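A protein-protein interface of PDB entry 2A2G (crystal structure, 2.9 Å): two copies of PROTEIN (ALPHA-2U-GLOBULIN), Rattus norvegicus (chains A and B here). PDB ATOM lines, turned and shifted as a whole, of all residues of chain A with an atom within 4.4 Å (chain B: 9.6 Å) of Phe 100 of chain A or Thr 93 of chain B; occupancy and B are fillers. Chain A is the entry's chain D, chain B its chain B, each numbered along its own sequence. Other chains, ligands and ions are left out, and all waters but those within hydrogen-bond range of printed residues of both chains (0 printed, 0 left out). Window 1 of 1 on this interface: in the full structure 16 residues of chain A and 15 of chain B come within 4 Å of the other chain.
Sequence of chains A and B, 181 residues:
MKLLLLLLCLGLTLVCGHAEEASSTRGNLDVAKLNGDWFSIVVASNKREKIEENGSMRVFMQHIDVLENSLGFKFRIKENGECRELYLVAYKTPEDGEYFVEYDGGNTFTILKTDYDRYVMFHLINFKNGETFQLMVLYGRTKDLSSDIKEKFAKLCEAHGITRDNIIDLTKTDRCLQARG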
ATOM      1  N   VAL A  89      21.527  19.378 -25.579  1.00  0.00           N
ATOM      2  CA  VAL A  89      21.116  20.774 -25.610  1.00  0.00           C
ATOM      3  C   VAL A  89      21.278  21.329 -24.197  1.00  0.00           C
ATOM      4  O   VAL A  89      20.852  20.712 -23.219  1.00  0.00           O
ATOM      5  CB  VAL A  89      19.644  20.939 -26.068  1.00  0.00           C
ATOM      6  CG1 VAL A  89      19.215  22.397 -25.952  1.00  0.00           C
ATOM      7  CG2 VAL A  89      19.484  20.468 -27.507  1.00  0.00           C
ATOM      8  N   ALA A  90      21.975  22.454 -24.099  1.00  0.00           N
ATOM      9  CA  ALA A  90      22.204  23.126 -22.827  1.00  0.00           C
ATOM     10  C   ALA A  90      21.398  24.415 -22.866  1.00  0.00           C
ATOM     11  O   ALA A  90      21.457  25.154 -23.847  1.00  0.00           O
ATOM     12  CB  ALA A  90      23.687  23.432 -22.644  1.00  0.00           C
ATOM     13  N   TYR A  91      20.654  24.690 -21.801  1.00  0.00           N
ATOM     14  CA  TYR A  91      19.825  25.888 -21.746  1.00  0.00           C
ATOM     15  C   TYR A  91      20.436  27.018 -20.932  1.00  0.00           C
ATOM     16  O   TYR A  91      20.983  26.801 -19.846  1.00  0.00           O
ATOM     17  CB  TYR A  91      18.448  25.540 -21.185  1.00  0.00           C
ATOM     18  CG  TYR A  91      17.779  24.415 -21.938  1.00  0.00           C
ATOM     19  CD1 TYR A  91      17.052  24.666 -23.101  1.00  0.00           C
ATOM     20  CD2 TYR A  91      17.904  23.093 -21.509  1.00  0.00           C
ATOM     21  CE1 TYR A  91      16.470  23.632 -23.822  1.00  0.00           C
ATOM     22  CE2 TYR A  91      17.325  22.051 -22.226  1.00  0.00           C
ATOM     23  CZ  TYR A  91      16.611  22.330 -23.381  1.00  0.00           C
ATOM     24  OH  TYR A  91      16.054  21.302 -24.107  1.00  0.00           O
ATOM     25  N   THR A  93      20.627  30.011 -18.465  1.00  0.00           N
ATOM     26  CA  THR A  93      19.926  30.253 -17.206  1.00  0.00           C
ATOM     27  C   THR A  93      19.970  31.744 -16.866  1.00  0.00           C
ATOM     28  O   THR A  93      20.643  32.524 -17.550  1.00  0.00           O
ATOM     29  CB  THR A  93      20.554  29.428 -16.057  1.00  0.00           C
ATOM     30  OG1 THR A  93      21.844  29.954 -15.739  1.00  0.00           O
ATOM     31  CG2 THR A  93      20.705  27.968 -16.458  1.00  0.00           C
ATOM     32  N   TYR A  99      24.880  28.098 -18.086  1.00  0.00           N
ATOM     33  CA  TYR A  99      24.082  27.180 -18.889  1.00  0.00           C
ATOM     34  C   TYR A  99      23.861  25.906 -18.100  1.00  0.00           C
ATOM     35  O   TYR A  99      24.699  25.520 -17.279  1.00  0.00           O
ATOM     36  CB  TYR A  99      24.810  26.817 -20.184  1.00  0.00           C
ATOM     37  CG  TYR A  99      24.819  27.883 -21.250  1.00  0.00           C
ATOM     38  CD1 TYR A  99      25.748  28.922 -21.221  1.00  0.00           C
ATOM     39  CD2 TYR A  99      23.911  27.840 -22.304  1.00  0.00           C
ATOM     40  CE1 TYR A  99      25.776  29.891 -22.216  1.00  0.00           C
ATOM     41  CE2 TYR A  99      23.928  28.805 -23.306  1.00  0.00           C
ATOM     42  CZ  TYR A  99      24.866  29.828 -23.257  1.00  0.00           C
ATOM     43  OH  TYR A  99      24.897  30.795 -24.238  1.00  0.00           O
ATOM     44  N   PHE A 100      22.726  25.261 -18.346  1.00  0.00           N
ATOM     45  CA  PHE A 100      22.431  24.008 -17.675  1.00  0.00           C
ATOM     46  C   PHE A 100      22.288  22.892 -18.693  1.00  0.00           C
ATOM     47  O   PHE A 100      21.835  23.107 -19.816  1.00  0.00           O
ATOM     48  CB  PHE A 100      21.151  24.092 -16.841  1.00  0.00           C
ATOM     49  CG  PHE A 100      20.794  22.795 -16.160  1.00  0.00           C
ATOM     50  CD1 PHE A 100      21.319  22.478 -14.911  1.00  0.00           C
ATOM     51  CD2 PHE A 100      19.993  21.861 -16.805  1.00  0.00           C
ATOM     52  CE1 PHE A 100      21.045  21.249 -14.309  1.00  0.00           C
ATOM     53  CE2 PHE A 100      19.713  20.632 -16.215  1.00  0.00           C
ATOM     54  CZ  PHE A 100      20.246  20.322 -14.966  1.00  0.00           C
ATOM     55  N   VAL A 101      22.697  21.701 -18.283  1.00  0.00           N
ATOM     56  CA  VAL A 101      22.606  20.520 -19.124  1.00  0.00           C
ATOM     57  C   VAL A 101      22.545  19.290 -18.230  1.00  0.00           C
ATOM     58  O   VAL A 101      23.298  19.172 -17.265  1.00  0.00           O
ATOM     59  CB  VAL A 101      23.799  20.419 -20.124  1.00  0.00           C
ATOM     60  CG1 VAL A 101      25.117  20.238 -19.385  1.00  0.00           C
ATOM     61  CG2 VAL A 101      23.571  19.278 -21.111  1.00  0.00           C
ATOM     62  N   GLU A 102      21.584  18.418 -18.508  1.00  0.00           N
ATOM     63  CA  GLU A 102      21.445  17.198 -17.740  1.00  0.00           C
ATOM     64  C   GLU A 102      22.249  16.134 -18.470  1.00  0.00           C
ATOM     65  O   GLU A 102      21.962  15.806 -19.624  1.00  0.00           O
ATOM     66  CB  GLU A 102      19.974  16.787 -17.629  1.00  0.00           C
ATOM     67  CG  GLU A 102      19.728  15.570 -16.733  1.00  0.00           C
ATOM     68  CD  GLU A 102      20.088  15.800 -15.270  1.00  0.00           C
ATOM     69  OE1 GLU A 102      20.122  16.965 -14.821  1.00  0.00           O
ATOM     70  OE2 GLU A 102      20.326  14.799 -14.560  1.00  0.00           O
ATOM     71  N   GLY A 106      23.256  16.797 -12.845  1.00  0.00           N
ATOM     72  CA  GLY A 106      22.920  18.164 -13.192  1.00  0.00           C
ATOM     73  C   GLY A 106      24.199  18.943 -13.435  1.00  0.00           C
ATOM     74  O   GLY A 106      25.070  18.992 -12.565  1.00  0.00           O
ATOM     75  N   ASN A 107      24.318  19.557 -14.610  1.00  0.00           N
ATOM     76  CA  ASN A 107      25.519  20.321 -14.936  1.00  0.00           C
ATOM     77  C   ASN A 107      25.274  21.799 -15.185  1.00  0.00           C
ATOM     78  O   ASN A 107      24.291  22.193 -15.812  1.00  0.00           O
ATOM     79  CB  ASN A 107      26.230  19.736 -16.161  1.00  0.00           C
ATOM     80  CG  ASN A 107      26.700  18.310 -15.947  1.00  0.00           C
ATOM     81  OD1 ASN A 107      27.628  18.057 -15.183  1.00  0.00           O
ATOM     82  ND2 ASN A 107      26.073  17.373 -16.641  1.00  0.00           N
ATOM     83  N   THR A 108      26.189  22.608 -14.672  1.00  0.00           N
ATOM     84  CA  THR A 108      26.166  24.049 -14.840  1.00  0.00           C
ATOM     85  C   THR A 108      27.541  24.359 -15.414  1.00  0.00           C
ATOM     86  O   THR A 108      28.535  23.759 -15.000  1.00  0.00           O
ATOM     87  CB  THR A 108      25.980  24.772 -13.487  1.00  0.00           C
ATOM     88  OG1 THR A 108      24.584  24.862 -13.181  1.00  0.00           O
ATOM     89  CG2 THR A 108      26.587  26.164 -13.522  1.00  0.00           C
ATOM     90  N   PHE A 127      26.731  17.841 -10.576  1.00  0.00           N
ATOM     91  CA  PHE A 127      26.063  17.480  -9.333  1.00  0.00           C
ATOM     92  C   PHE A 127      25.320  16.176  -9.543  1.00  0.00           C
ATOM     93  O   PHE A 127      24.517  16.054 -10.468  1.00  0.00           O
ATOM     94  CB  PHE A 127      25.064  18.542  -8.865  1.00  0.00           C
ATOM     95  CG  PHE A 127      24.297  18.136  -7.637  1.00  0.00           C
ATOM     96  CD1 PHE A 127      24.878  18.224  -6.378  1.00  0.00           C
ATOM     97  CD2 PHE A 127      23.022  17.587  -7.748  1.00  0.00           C
ATOM     98  CE1 PHE A 127      24.201  17.780  -5.243  1.00  0.00           C
ATOM     99  CE2 PHE A 127      22.337  17.137  -6.622  1.00  0.00           C
ATOM    100  CZ  PHE A 127      22.929  17.228  -5.365  1.00  0.00           C
ATOM    101  N   GLU B  68      15.038  11.042  -9.027  1.00  0.00           N
ATOM    102  CA  GLU B  68      16.497  11.022  -8.945  1.00  0.00           C
ATOM    103  C   GLU B  68      17.075  12.378  -9.323  1.00  0.00           C
ATOM    104  O   GLU B  68      17.025  12.786 -10.485  1.00  0.00           O
ATOM    105  CB  GLU B  68      17.088   9.939  -9.857  1.00  0.00           C
ATOM    106  CG  GLU B  68      16.661   8.503  -9.536  1.00  0.00           C
ATOM    107  CD  GLU B  68      17.052   8.048  -8.139  1.00  0.00           C
ATOM    108  OE1 GLU B  68      16.494   8.577  -7.156  1.00  0.00           O
ATOM    109  OE2 GLU B  68      17.904   7.141  -8.023  1.00  0.00           O
ATOM    110  N   ASN B  69      17.617  13.068  -8.320  1.00  0.00           N
ATOM    111  CA  ASN B  69      18.218  14.389  -8.494  1.00  0.00           C
ATOM    112  C   ASN B  69      17.298  15.308  -9.295  1.00  0.00           C
ATOM    113  O   ASN B  69      17.756  16.143 -10.079  1.00  0.00           O
ATOM    114  CB  ASN B  69      19.581  14.272  -9.188  1.00  0.00           C
ATOM    115  CG  ASN B  69      20.554  13.394  -8.424  1.00  0.00           C
ATOM    116  OD1 ASN B  69      20.881  13.662  -7.271  1.00  0.00           O
ATOM    117  ND2 ASN B  69      21.034  12.345  -9.078  1.00  0.00           N
ATOM    118  N   SER B  70      15.995  15.145  -9.087  1.00  0.00           N
ATOM    119  CA  SER B  70      15.006  15.938  -9.800  1.00  0.00           C
ATOM    120  C   SER B  70      13.638  15.925  -9.135  1.00  0.00           C
ATOM    121  O   SER B  70      13.355  15.098  -8.265  1.00  0.00           O
ATOM    122  CB  SER B  70      14.875  15.438 -11.244  1.00  0.00           C
ATOM    123  OG  SER B  70      14.449  14.084 -11.292  1.00  0.00           O
ATOM    124  N   LEU B  71      12.801  16.869  -9.547  1.00  0.00           N
ATOM    125  CA  LEU B  71      11.446  16.995  -9.037  1.00  0.00           C
ATOM    126  C   LEU B  71      10.483  17.004 -10.216  1.00  0.00           C
ATOM    127  O   LEU B  71      10.718  17.687 -11.215  1.00  0.00           O
ATOM    128  CB  LEU B  71      11.291  18.289  -8.231  1.00  0.00           C
ATOM    129  CG  LEU B  71      12.005  18.386  -6.882  1.00  0.00           C
ATOM    130  CD1 LEU B  71      11.865  19.797  -6.333  1.00  0.00           C
ATOM    131  CD2 LEU B  71      11.423  17.371  -5.913  1.00  0.00           C
ATOM    132  N   VAL B  89       9.763  18.118 -15.448  1.00  0.00           N
ATOM    133  CA  VAL B  89      10.828  17.602 -14.601  1.00  0.00           C
ATOM    134  C   VAL B  89      11.857  18.716 -14.430  1.00  0.00           C
ATOM    135  O   VAL B  89      12.266  19.358 -15.401  1.00  0.00           O
ATOM    136  CB  VAL B  89      11.511  16.354 -15.217  1.00  0.00           C
ATOM    137  CG1 VAL B  89      12.705  15.932 -14.368  1.00  0.00           C
ATOM    138  CG2 VAL B  89      10.518  15.203 -15.314  1.00  0.00           C
ATOM    139  N   ALA B  90      12.199  18.997 -13.179  1.00  0.00           N
ATOM    140  CA  ALA B  90      13.181  20.018 -12.845  1.00  0.00           C
ATOM    141  C   ALA B  90      14.401  19.286 -12.308  1.00  0.00           C
ATOM    142  O   ALA B  90      14.272  18.409 -11.457  1.00  0.00           O
ATOM    143  CB  ALA B  90      12.625  20.970 -11.790  1.00  0.00           C
ATOM    144  N   TYR B  91      15.581  19.651 -12.795  1.00  0.00           N
ATOM    145  CA  TYR B  91      16.812  18.997 -12.364  1.00  0.00           C
ATOM    146  C   TYR B  91      17.602  19.793 -11.338  1.00  0.00           C
ATOM    147  O   TYR B  91      17.760  21.011 -11.460  1.00  0.00           O
ATOM    148  CB  TYR B  91      17.693  18.704 -13.577  1.00  0.00           C
ATOM    149  CG  TYR B  91      16.973  17.922 -14.648  1.00  0.00           C
ATOM    150  CD1 TYR B  91      16.894  16.530 -14.585  1.00  0.00           C
ATOM    151  CD2 TYR B  91      16.338  18.573 -15.704  1.00  0.00           C
ATOM    152  CE1 TYR B  91      16.198  15.808 -15.544  1.00  0.00           C
ATOM    153  CE2 TYR B  91      15.636  17.856 -16.668  1.00  0.00           C
ATOM    154  CZ  TYR B  91      15.571  16.475 -16.580  1.00  0.00           C
ATOM    155  OH  TYR B  91      14.860  15.760 -17.517  1.00  0.00           O
ATOM    156  N   LYS B  92      18.095  19.089 -10.325  1.00  0.00           N
ATOM    157  CA  LYS B  92      18.900  19.699  -9.279  1.00  0.00           C
ATOM    158  C   LYS B  92      20.207  20.148  -9.926  1.00  0.00           C
ATOM    159  O   LYS B  92      20.748  19.464 -10.805  1.00  0.00           O
ATOM    160  CB  LYS B  92      19.187  18.684  -8.166  1.00  0.00           C
ATOM    161  CG  LYS B  92      19.951  19.250  -6.973  1.00  0.00           C
ATOM    162  CD  LYS B  92      19.167  20.351  -6.270  1.00  0.00           C
ATOM    163  CE  LYS B  92      19.870  20.823  -5.004  1.00  0.00           C
ATOM    164  NZ  LYS B  92      21.148  21.518  -5.297  1.00  0.00           N
ATOM    165  N   THR B  93      20.679  21.322  -9.529  1.00  0.00           N
ATOM    166  CA  THR B  93      21.923  21.870 -10.066  1.00  0.00           C
ATOM    167  C   THR B  93      22.992  21.896  -8.971  1.00  0.00           C
ATOM    168  O   THR B  93      22.704  21.603  -7.806  1.00  0.00           O
ATOM    169  CB  THR B  93      21.701  23.295 -10.624  1.00  0.00           C
ATOM    170  OG1 THR B  93      21.464  24.203  -9.546  1.00  0.00           O
ATOM    171  CG2 THR B  93      20.506  23.329 -11.565  1.00  0.00           C
ATOM    172  N   PRO B  94      24.255  22.181  -9.343  1.00  0.00           N
ATOM    173  CA  PRO B  94      25.340  22.231  -8.361  1.00  0.00           C
ATOM    174  C   PRO B  94      25.231  23.404  -7.377  1.00  0.00           C
ATOM    175  O   PRO B  94      25.866  23.391  -6.326  1.00  0.00           O
ATOM    176  CB  PRO B  94      26.578  22.375  -9.243  1.00  0.00           C
ATOM    177  CG  PRO B  94      26.177  21.665 -10.500  1.00  0.00           C
ATOM    178  CD  PRO B  94      24.798  22.202 -10.711  1.00  0.00           C
ATOM    179  N   GLU B  95      24.486  24.452  -7.752  1.00  0.00           N
ATOM    180  CA  GLU B  95      24.316  25.621  -6.881  1.00  0.00           C
ATOM    181  C   GLU B  95      23.325  25.224  -5.789  1.00  0.00           C
ATOM    182  O   GLU B  95      22.152  25.005  -6.075  1.00  0.00           O
ATOM    183  CB  GLU B  95      23.761  26.824  -7.664  1.00  0.00           C
ATOM    184  CG  GLU B  95      23.740  26.683  -9.195  1.00  0.00           C
ATOM    185  CD  GLU B  95      25.123  26.682  -9.819  1.00  0.00           C
ATOM    186  OE1 GLU B  95      25.817  27.715  -9.734  1.00  0.00           O
ATOM    187  OE2 GLU B  95      25.508  25.654 -10.413  1.00  0.00           O
ATOM    188  N   ASP B  96      23.796  25.148  -4.542  1.00  0.00           N
ATOM    189  CA  ASP B  96      22.977  24.738  -3.392  1.00  0.00           C
ATOM    190  C   ASP B  96      21.499  25.133  -3.359  1.00  0.00           C
ATOM    191  O   ASP B  96      21.149  26.310  -3.277  1.00  0.00           O
ATOM    192  CB  ASP B  96      23.637  25.158  -2.074  1.00  0.00           C
ATOM    193  CG  ASP B  96      22.819  24.743  -0.856  1.00  0.00           C
ATOM    194  OD1 ASP B  96      22.471  23.549  -0.751  1.00  0.00           O
ATOM    195  OD2 ASP B  96      22.524  25.614  -0.009  1.00  0.00           O
ATOM    196  N   GLY B  97      20.648  24.108  -3.374  1.00  0.00           N
ATOM    197  CA  GLY B  97      19.210  24.296  -3.313  1.00  0.00           C
ATOM    198  C   GLY B  97      18.547  24.720  -4.607  1.00  0.00           C
ATOM    199  O   GLY B  97      17.330  24.891  -4.650  1.00  0.00           O
ATOM    200  N   GLU B  98      19.337  24.874  -5.665  1.00  0.00           N
ATOM    201  CA  GLU B  98      18.815  25.299  -6.962  1.00  0.00           C
ATOM    202  C   GLU B  98      18.391  24.180  -7.904  1.00  0.00           C
ATOM    203  O   GLU B  98      19.040  23.137  -7.997  1.00  0.00           O
ATOM    204  CB  GLU B  98      19.840  26.183  -7.674  1.00  0.00           C
ATOM    205  CG  GLU B  98      19.428  27.635  -7.818  1.00  0.00           C
ATOM    206  CD  GLU B  98      20.411  28.440  -8.645  1.00  0.00           C
ATOM    207  OE1 GLU B  98      20.726  28.027  -9.782  1.00  0.00           O
ATOM    208  OE2 GLU B  98      20.860  29.495  -8.162  1.00  0.00           O
ATOM    209  N   TYR B  99      17.308  24.438  -8.627  1.00  0.00           N
ATOM    210  CA  TYR B  99      16.759  23.503  -9.600  1.00  0.00           C
ATOM    211  C   TYR B  99      16.548  24.230 -10.911  1.00  0.00           C
ATOM    212  O   TYR B  99      16.292  25.439 -10.927  1.00  0.00           O
ATOM    213  CB  TYR B  99      15.406  22.963  -9.133  1.00  0.00           C
ATOM    214  CG  TYR B  99      15.459  21.929  -8.037  1.00  0.00           C
ATOM    215  CD1 TYR B  99      15.577  22.305  -6.699  1.00  0.00           C
ATOM    216  CD2 TYR B  99      15.365  20.572  -8.335  1.00  0.00           C
ATOM    217  CE1 TYR B  99      15.598  21.355  -5.684  1.00  0.00           C
ATOM    218  CE2 TYR B  99      15.385  19.613  -7.328  1.00  0.00           C
ATOM    219  CZ  TYR B  99      15.501  20.011  -6.002  1.00  0.00           C
ATOM    220  OH  TYR B  99      15.527  19.077  -4.992  1.00  0.00           O
ATOM    221  N   PHE B 100      16.665  23.492 -12.010  1.00  0.00           N
ATOM    222  CA  PHE B 100      16.445  24.081 -13.319  1.00  0.00           C
ATOM    223  C   PHE B 100      15.283  23.391 -14.010  1.00  0.00           C
ATOM    224  O   PHE B 100      15.049  22.198 -13.827  1.00  0.00           O
ATOM    225  CB  PHE B 100      17.685  23.984 -14.207  1.00  0.00           C
ATOM    226  CG  PHE B 100      17.477  24.552 -15.589  1.00  0.00           C
ATOM    227  CD1 PHE B 100      17.678  25.906 -15.841  1.00  0.00           C
ATOM    228  CD2 PHE B 100      17.008  23.743 -16.618  1.00  0.00           C
ATOM    229  CE1 PHE B 100      17.421  26.446 -17.102  1.00  0.00           C
ATOM    230  CE2 PHE B 100      16.746  24.271 -17.878  1.00  0.00           C
ATOM    231  CZ  PHE B 100      16.948  25.629 -18.119  1.00  0.00           C
ATOM    232  N   VAL B 101      14.554  24.168 -14.796  1.00  0.00           N
ATOM    233  CA  VAL B 101      13.421  23.661 -15.552  1.00  0.00           C
ATOM    234  C   VAL B 101      13.204  24.558 -16.762  1.00  0.00           C
ATOM    235  O   VAL B 101      13.239  25.783 -16.656  1.00  0.00           O
ATOM    236  CB  VAL B 101      12.128  23.579 -14.686  1.00  0.00           C
ATOM    237  CG1 VAL B 101      11.678  24.963 -14.242  1.00  0.00           C
ATOM    238  CG2 VAL B 101      11.016  22.870 -15.453  1.00  0.00           C
ATOM    239  N   GLU B 102      13.067  23.937 -17.927  1.00  0.00           N
ATOM    240  CA  GLU B 102      12.830  24.687 -19.143  1.00  0.00           C
ATOM    241  C   GLU B 102      11.321  24.766 -19.316  1.00  0.00           C
ATOM    242  O   GLU B 102      10.646  23.742 -19.449  1.00  0.00           O
ATOM    243  CB  GLU B 102      13.478  23.996 -20.346  1.00  0.00           C
ATOM    244  CG  GLU B 102      13.375  24.783 -21.655  1.00  0.00           C
ATOM    245  CD  GLU B 102      14.121  26.112 -21.634  1.00  0.00           C
ATOM    246  OE1 GLU B 102      15.059  26.278 -20.825  1.00  0.00           O
ATOM    247  OE2 GLU B 102      13.772  26.994 -22.447  1.00  0.00           O
ATOM    248  N   GLY B 106      14.270  29.696 -19.623  1.00  0.00           N
ATOM    249  CA  GLY B 106      15.100  28.979 -18.674  1.00  0.00           C
ATOM    250  C   GLY B 106      14.710  29.387 -17.267  1.00  0.00           C
ATOM    251  O   GLY B 106      14.726  30.575 -16.939  1.00  0.00           O
ATOM    252  N   ASN B 107      14.364  28.413 -16.429  1.00  0.00           N
ATOM    253  CA  ASN B 107      13.965  28.714 -15.056  1.00  0.00           C
ATOM    254  C   ASN B 107      14.865  28.107 -13.994  1.00  0.00           C
ATOM    255  O   ASN B 107      15.316  26.967 -14.104  1.00  0.00           O
ATOM    256  CB  ASN B 107      12.526  28.260 -14.788  1.00  0.00           C
ATOM    257  CG  ASN B 107      11.510  28.961 -15.671  1.00  0.00           C
ATOM    258  OD1 ASN B 107      11.252  30.151 -15.516  1.00  0.00           O
ATOM    259  ND2 ASN B 107      10.914  28.214 -16.587  1.00  0.00           N
ATOM    260  N   THR B 108      15.120  28.899 -12.963  1.00  0.00           N
ATOM    261  CA  THR B 108      15.915  28.492 -11.821  1.00  0.00           C
ATOM    262  C   THR B 108      15.003  28.779 -10.637  1.00  0.00           C
ATOM    263  O   THR B 108      14.303  29.794 -10.625  1.00  0.00           O
ATOM    264  CB  THR B 108      17.210  29.328 -11.707  1.00  0.00           C
ATOM    265  OG1 THR B 108      18.228  28.745 -12.528  1.00  0.00           O
ATOM    266  CG2 THR B 108      17.691  29.401 -10.270  1.00  0.00           C
ATOM    267  N   PHE B 109      14.946  27.860  -9.681  1.00  0.00           N
ATOM    268  CA  PHE B 109      14.096  28.076  -8.520  1.00  0.00           C
ATOM    269  C   PHE B 109      14.630  27.387  -7.279  1.00  0.00           C
ATOM    270  O   PHE B 109      15.453  26.470  -7.364  1.00  0.00           O
ATOM    271  CB  PHE B 109      12.659  27.613  -8.805  1.00  0.00           C
ATOM    272  CG  PHE B 109      12.481  26.116  -8.833  1.00  0.00           C
ATOM    273  CD1 PHE B 109      12.443  25.375  -7.653  1.00  0.00           C
ATOM    274  CD2 PHE B 109      12.322  25.448 -10.041  1.00  0.00           C
ATOM    275  CE1 PHE B 109      12.241  23.997  -7.676  1.00  0.00           C
ATOM    276  CE2 PHE B 109      12.118  24.069 -10.076  1.00  0.00           C
ATOM    277  CZ  PHE B 109      12.081  23.342  -8.889  1.00  0.00           C
ATOM    278  N   THR B 110      14.156  27.841  -6.125  1.00  0.00           N
ATOM    279  CA  THR B 110      14.548  27.264  -4.847  1.00  0.00           C
ATOM    280  C   THR B 110      13.352  27.258  -3.905  1.00  0.00           C
ATOM    281  O   THR B 110      12.420  28.055  -4.048  1.00  0.00           O
ATOM    282  CB  THR B 110      15.692  28.057  -4.171  1.00  0.00           C
ATOM    283  OG1 THR B 110      15.304  29.427  -4.011  1.00  0.00           O
ATOM    284  CG2 THR B 110      16.969  27.999  -5.015  1.00  0.00           C
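OG1 of Thr 108 of chain A is in hydrogen-bond range of OE2 of Glu 95 of chain B, 3.0 Å away.
The backbone carbonyl oxygen of Asn 69 of chain B lies within hydrogen-bond range of the backbone NH of Lys 92 of chain B, at 3.0 Å. N of Phe 100 of chain B lies within hydrogen-bond range of O of Tyr 91 of chain B (2.8 Å). The backbone NH (N) of Thr 93 of chain B lies within hydrogen-bond range of the backbone carbonyl oxygen (O) of Glu 98 of chain B, at 2.9 Å. N of Phe 100 of chain A sits at hydrogen-bond distance from O of Tyr 91 of chain A, 2.8 Å away. The backbone carbonyl oxygen (O) of Phe 127 of chain A sits at hydrogen-bond distance from the backbone NH (N) of Gly 106 of chain A, at 2.8 Å.
Among the printed residues, pairs that only touch across the chains: Tyr 91 of chain A with Phe 100 of chain B (3.4 Å), Tyr 91 of chain A with Glu 102 of chain B (3.4 Å), Thr 93 of chain A with Phe 100 of chain B (3.7 Å), Phe 100 of chain A with Tyr 91 of chain B (3.3 Å), Phe 100 of chain A with Lys 92 of chain B (3.9 Å), Phe 100 of chain A with Thr 93 of chain B (3.5 Å), Phe 100 of chain A with Phe 100 of chain B (3.5 Å), Glu 102 of chain A with Tyr 91 of chain B (3.2 Å), Gly 106 of chain A with Lys 92 of chain B (3.5 Å), Gly 106 of chain A with Pro 94 of chain B (3.6 Å), Thr 108 of chain A with Pro 94 of chain B (3.6 Å), Phe 127 of chain A with Asn 69 of chain B (3.8 Å), Phe 127 of chain A with Lys 92 of chain B (3.2 Å), Phe 127 of chain A with Thr 93 of chain B (3.8 Å) and Phe 127 of chain A with Pro 94 of chain B (3.7 Å).
Of chain B, only Tyr 91, Lys 92, Thr 93 and Phe 100 come within 4 Å of Phe 100 of chain A. Thr 93 of chain B touches two residues of chain A. No residue of chain B comes within 4 Å of Val 101 of chain A. Of the printed residues of chain A, Asn 69 of chain B touches Phe 127 (3.8 Å). Of the printed residues of chain B, Glu 102 of chain A touches Tyr 91 (3.2 Å). Printed residues of chain A within 4 Å of Pro 94 of chain B: Gly 106, Thr 108 and Phe 127. Printed residues of chain B within 4 Å of Tyr 91 of chain A: Phe 100 and Glu 102. Of the printed residues of chain A, Tyr 91 of chain B touches Phe 100 (3.3 Å) and Glu 102 (3.2 Å).
Printed residues of chain B that touch a printed residue of chain A: Asn 69, Tyr 91, Lys 92, Thr 93, Pro 94, Glu 95, Phe 100 and Glu 102. Hydrophobic or aromatic side chains of chain B that line the printed part of chain A: Tyr 91, Pro 94 and Phe 100. Along chain A the printed residues that touch a printed residue of chain B span positions 91 to 127. Among the printed residues, 16 pairs touch across the chains.
Tyr 91 of chain A touches Phe 100 of chain B, and with the chains exchanged Phe 100 of chain A touches Tyr 91 of chain B. Tyr 91 of chain A touches Glu 102 of chain B, and with the chains exchanged Glu 102 of chain A touches Tyr 91 of chain B. Thr 93 of chain A touches Phe 100 of chain B, and with the chains exchanged Phe 100 of chain A touches Thr 93 of chain B. Phe 100 of chain A touches its own counterpart, Phe 100 of chain B. 11 positions are printed for both chains. Of the 16 pairs that touch across the chains among the printed residues, 7 have their exchanged pair printed and touching as well.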
